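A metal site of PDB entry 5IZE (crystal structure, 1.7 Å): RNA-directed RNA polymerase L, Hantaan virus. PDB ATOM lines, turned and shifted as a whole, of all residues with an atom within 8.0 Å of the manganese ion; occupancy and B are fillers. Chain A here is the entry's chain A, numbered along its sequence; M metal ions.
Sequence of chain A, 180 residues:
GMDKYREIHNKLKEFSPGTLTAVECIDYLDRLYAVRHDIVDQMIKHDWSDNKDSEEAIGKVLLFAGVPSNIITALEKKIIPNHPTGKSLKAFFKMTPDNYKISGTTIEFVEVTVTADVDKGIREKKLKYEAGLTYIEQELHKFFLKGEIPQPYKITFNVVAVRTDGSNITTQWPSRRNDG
A ring nitrogen (ND1) of His 9 lies within hydrogen-bond range of the side-chain amide oxygen of Asn 10 (2.8 Å).
The nearest printed residue that does not touch the manganese ion is Thr 19 (4.3 Å).
The side-chain hydroxyl (OG) of Ser 16 is bound to the manganese ion (2.1 Å).
The manganese ion is bound by NE2 of His 9, at 2.3 Å.
O of Gly 18 is bound to the manganese ion (2.4 Å).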
ATOM      1  N   HIS A   9      13.642  -9.132   2.786  1.00  0.00           N
ATOM      2  CA  HIS A   9      13.954  -8.763   1.404  1.00  0.00           C
ATOM      3  C   HIS A   9      14.745  -9.881   0.717  1.00  0.00           C
ATOM      4  O   HIS A   9      14.432 -10.254  -0.406  1.00  0.00           O
ATOM      5  CB  HIS A   9      14.774  -7.461   1.350  1.00  0.00           C
ATOM      6  CG  HIS A   9      15.325  -7.169   0.002  1.00  0.00           C
ATOM      7  ND1 HIS A   9      16.513  -7.708  -0.445  1.00  0.00           N
ATOM      8  CD2 HIS A   9      14.835  -6.454  -1.043  1.00  0.00           C
ATOM      9  CE1 HIS A   9      16.735  -7.324  -1.685  1.00  0.00           C
ATOM     10  NE2 HIS A   9      15.734  -6.567  -2.066  1.00  0.00           N
ATOM     11  N   ASN A  10      15.736 -10.417   1.402  1.00  0.00           N
ATOM     12  CA  ASN A  10      16.600 -11.430   0.784  1.00  0.00           C
ATOM     13  C   ASN A  10      15.921 -12.776   0.553  1.00  0.00           C
ATOM     14  O   ASN A  10      16.383 -13.572  -0.261  1.00  0.00           O
ATOM     15  CB  ASN A  10      17.909 -11.553   1.563  1.00  0.00           C
ATOM     16  CG  ASN A  10      18.768 -10.301   1.411  1.00  0.00           C
ATOM     17  OD1 ASN A  10      18.495  -9.437   0.558  1.00  0.00           O
ATOM     18  ND2 ASN A  10      19.786 -10.187   2.236  1.00  0.00           N
ATOM     19  N   LEU A  12      12.850 -12.733  -0.776  1.00  0.00           N
ATOM     20  CA  LEU A  12      11.989 -12.479  -1.926  1.00  0.00           C
ATOM     21  C   LEU A  12      12.544 -13.092  -3.211  1.00  0.00           C
ATOM     22  O   LEU A  12      11.780 -13.483  -4.094  1.00  0.00           O
ATOM     23  CB  LEU A  12      11.734 -10.979  -2.114  1.00  0.00           C
ATOM     24  CG  LEU A  12      10.941 -10.297  -0.997  1.00  0.00           C
ATOM     25  CD1 LEU A  12      10.907  -8.781  -1.179  1.00  0.00           C
ATOM     26  CD2 LEU A  12       9.512 -10.817  -0.945  1.00  0.00           C
ATOM     27  N   LYS A  13      13.879 -13.178  -3.297  1.00  0.00           N
ATOM     28  CA  LYS A  13      14.585 -13.904  -4.379  1.00  0.00           C
ATOM     29  C   LYS A  13      14.178 -13.336  -5.747  1.00  0.00           C
ATOM     30  O   LYS A  13      14.426 -12.164  -5.990  1.00  0.00           O
ATOM     31  CB  LYS A  13      14.374 -15.421  -4.256  1.00  0.00           C
ATOM     32  CG  LYS A  13      14.758 -16.018  -2.889  1.00  0.00           C
ATOM     33  CD  LYS A  13      14.381 -17.493  -2.756  1.00  0.00           C
ATOM     34  CE  LYS A  13      12.880 -17.749  -2.589  1.00  0.00           C
ATOM     35  NZ  LYS A  13      12.259 -18.214  -3.851  1.00  0.00           N
ATOM     36  N   PHE A  15      11.410 -12.234  -6.816  1.00  0.00           N
ATOM     37  CA  PHE A  15      10.487 -11.087  -6.693  1.00  0.00           C
ATOM     38  C   PHE A  15      11.113  -9.810  -6.148  1.00  0.00           C
ATOM     39  O   PHE A  15      10.454  -8.779  -6.102  1.00  0.00           O
ATOM     40  CB  PHE A  15       9.246 -11.495  -5.894  1.00  0.00           C
ATOM     41  CG  PHE A  15       8.444 -12.541  -6.567  1.00  0.00           C
ATOM     42  CD1 PHE A  15       8.028 -12.384  -7.878  1.00  0.00           C
ATOM     43  CD2 PHE A  15       8.134 -13.716  -5.914  1.00  0.00           C
ATOM     44  CE1 PHE A  15       7.294 -13.359  -8.523  1.00  0.00           C
ATOM     45  CE2 PHE A  15       7.403 -14.708  -6.552  1.00  0.00           C
ATOM     46  CZ  PHE A  15       6.988 -14.537  -7.846  1.00  0.00           C
ATOM     47  N   SER A  16      12.378  -9.863  -5.740  1.00  0.00           N
ATOM     48  CA  SER A  16      13.169  -8.652  -5.598  1.00  0.00           C
ATOM     49  C   SER A  16      14.626  -8.964  -5.913  1.00  0.00           C
ATOM     50  O   SER A  16      15.422  -9.189  -5.008  1.00  0.00           O
ATOM     51  CB  SER A  16      12.980  -8.003  -4.228  1.00  0.00           C
ATOM     52  OG  SER A  16      13.477  -6.683  -4.275  1.00  0.00           O
ATOM     53  N   PRO A  17      14.963  -9.017  -7.215  1.00  0.00           N
ATOM     54  CA  PRO A  17      16.267  -9.520  -7.616  1.00  0.00           C
ATOM     55  C   PRO A  17      17.436  -8.579  -7.360  1.00  0.00           C
ATOM     56  O   PRO A  17      18.584  -9.016  -7.425  1.00  0.00           O
ATOM     57  CB  PRO A  17      16.085  -9.795  -9.121  1.00  0.00           C
ATOM     58  CG  PRO A  17      15.079  -8.775  -9.544  1.00  0.00           C
ATOM     59  CD  PRO A  17      14.125  -8.674  -8.387  1.00  0.00           C
ATOM     60  N   GLY A  18      17.174  -7.311  -7.056  1.00  0.00           N
ATOM     61  CA  GLY A  18      18.223  -6.364  -6.689  1.00  0.00           C
ATOM     62  C   GLY A  18      18.445  -6.302  -5.185  1.00  0.00           C
ATOM     63  O   GLY A  18      17.481  -6.296  -4.419  1.00  0.00           O
ATOM     64  N   THR A  19      19.710  -6.252  -4.769  1.00  0.00           N
ATOM     65  CA  THR A  19      20.101  -5.944  -3.387  1.00  0.00           C
ATOM     66  C   THR A  19      19.346  -4.716  -2.849  1.00  0.00           C
ATOM     67  O   THR A  19      19.105  -3.747  -3.570  1.00  0.00           O
ATOM     68  CB  THR A  19      21.606  -5.651  -3.310  1.00  0.00           C
ATOM     69  OG1 THR A  19      22.323  -6.798  -3.784  1.00  0.00           O
ATOM     70  CG2 THR A  19      22.073  -5.334  -1.899  1.00  0.00           C
ATOM     71  N   LEU A  20      18.966  -4.759  -1.585  1.00  0.00           N
ATOM     72  CA  LEU A  20      18.280  -3.635  -0.940  1.00  0.00           C
ATOM     73  C   LEU A  20      19.126  -2.365  -1.055  1.00  0.00           C
ATOM     74  O   LEU A  20      20.318  -2.389  -0.742  1.00  0.00           O
ATOM     75  CB  LEU A  20      18.040  -3.991   0.529  1.00  0.00           C
ATOM     76  CG  LEU A  20      17.074  -3.192   1.364  1.00  0.00           C
ATOM     77  CD1 LEU A  20      15.664  -3.282   0.801  1.00  0.00           C
ATOM     78  CD2 LEU A  20      17.128  -3.727   2.790  1.00  0.00           C
ATOM     79  N   THR A  21      18.519  -1.262  -1.513  1.00  0.00           N
ATOM     80  CA  THR A  21      19.217   0.036  -1.663  1.00  0.00           C
ATOM     81  C   THR A  21      19.080   0.974  -0.453  1.00  0.00           C
ATOM     82  O   THR A  21      18.154   0.840   0.354  1.00  0.00           O
ATOM     83  CB  THR A  21      18.721   0.761  -2.910  1.00  0.00           C
ATOM     84  OG1 THR A  21      17.355   1.179  -2.743  1.00  0.00           O
ATOM     85  CG2 THR A  21      18.822  -0.150  -4.150  1.00  0.00           C
ATOM     86  N   GLU A  24      15.761   2.986  -0.655  1.00  0.00           N
ATOM     87  CA  GLU A  24      14.666   2.111  -0.191  1.00  0.00           C
ATOM     88  C   GLU A  24      14.561   2.095   1.301  1.00  0.00           C
ATOM     89  O   GLU A  24      13.476   2.304   1.857  1.00  0.00           O
ATOM     90  CB  GLU A  24      14.882   0.665  -0.618  1.00  0.00           C
ATOM     91  CG  GLU A  24      14.330   0.312  -1.942  1.00  0.00           C
ATOM     92  CD  GLU A  24      14.576  -1.146  -2.217  1.00  0.00           C
ATOM     93  OE1 GLU A  24      15.736  -1.508  -2.482  1.00  0.00           O
ATOM     94  OE2 GLU A  24      13.621  -1.921  -2.083  1.00  0.00           O
ATOM     95  N   TYR A  28      11.596   3.135   3.802  1.00  0.00           N
ATOM     96  CA  TYR A  28      10.950   2.146   4.695  1.00  0.00           C
ATOM     97  C   TYR A  28      11.026   2.601   6.144  1.00  0.00           C
ATOM     98  O   TYR A  28      10.040   2.472   6.889  1.00  0.00           O
ATOM     99  CB  TYR A  28      11.499   0.743   4.483  1.00  0.00           C
ATOM    100  CG  TYR A  28      11.469   0.263   3.033  1.00  0.00           C
ATOM    101  CD1 TYR A  28      10.536   0.758   2.120  1.00  0.00           C
ATOM    102  CD2 TYR A  28      12.364  -0.700   2.583  1.00  0.00           C
ATOM    103  CE1 TYR A  28      10.530   0.337   0.802  1.00  0.00           C
ATOM    104  CE2 TYR A  28      12.354  -1.149   1.275  1.00  0.00           C
ATOM    105  CZ  TYR A  28      11.431  -0.620   0.381  1.00  0.00           C
ATOM    106  OH  TYR A  28      11.396  -1.048  -0.929  1.00  0.00           O
HETATM  107 MN    MN M   1      15.214  -5.459  -4.052  1.00  0.00          MN
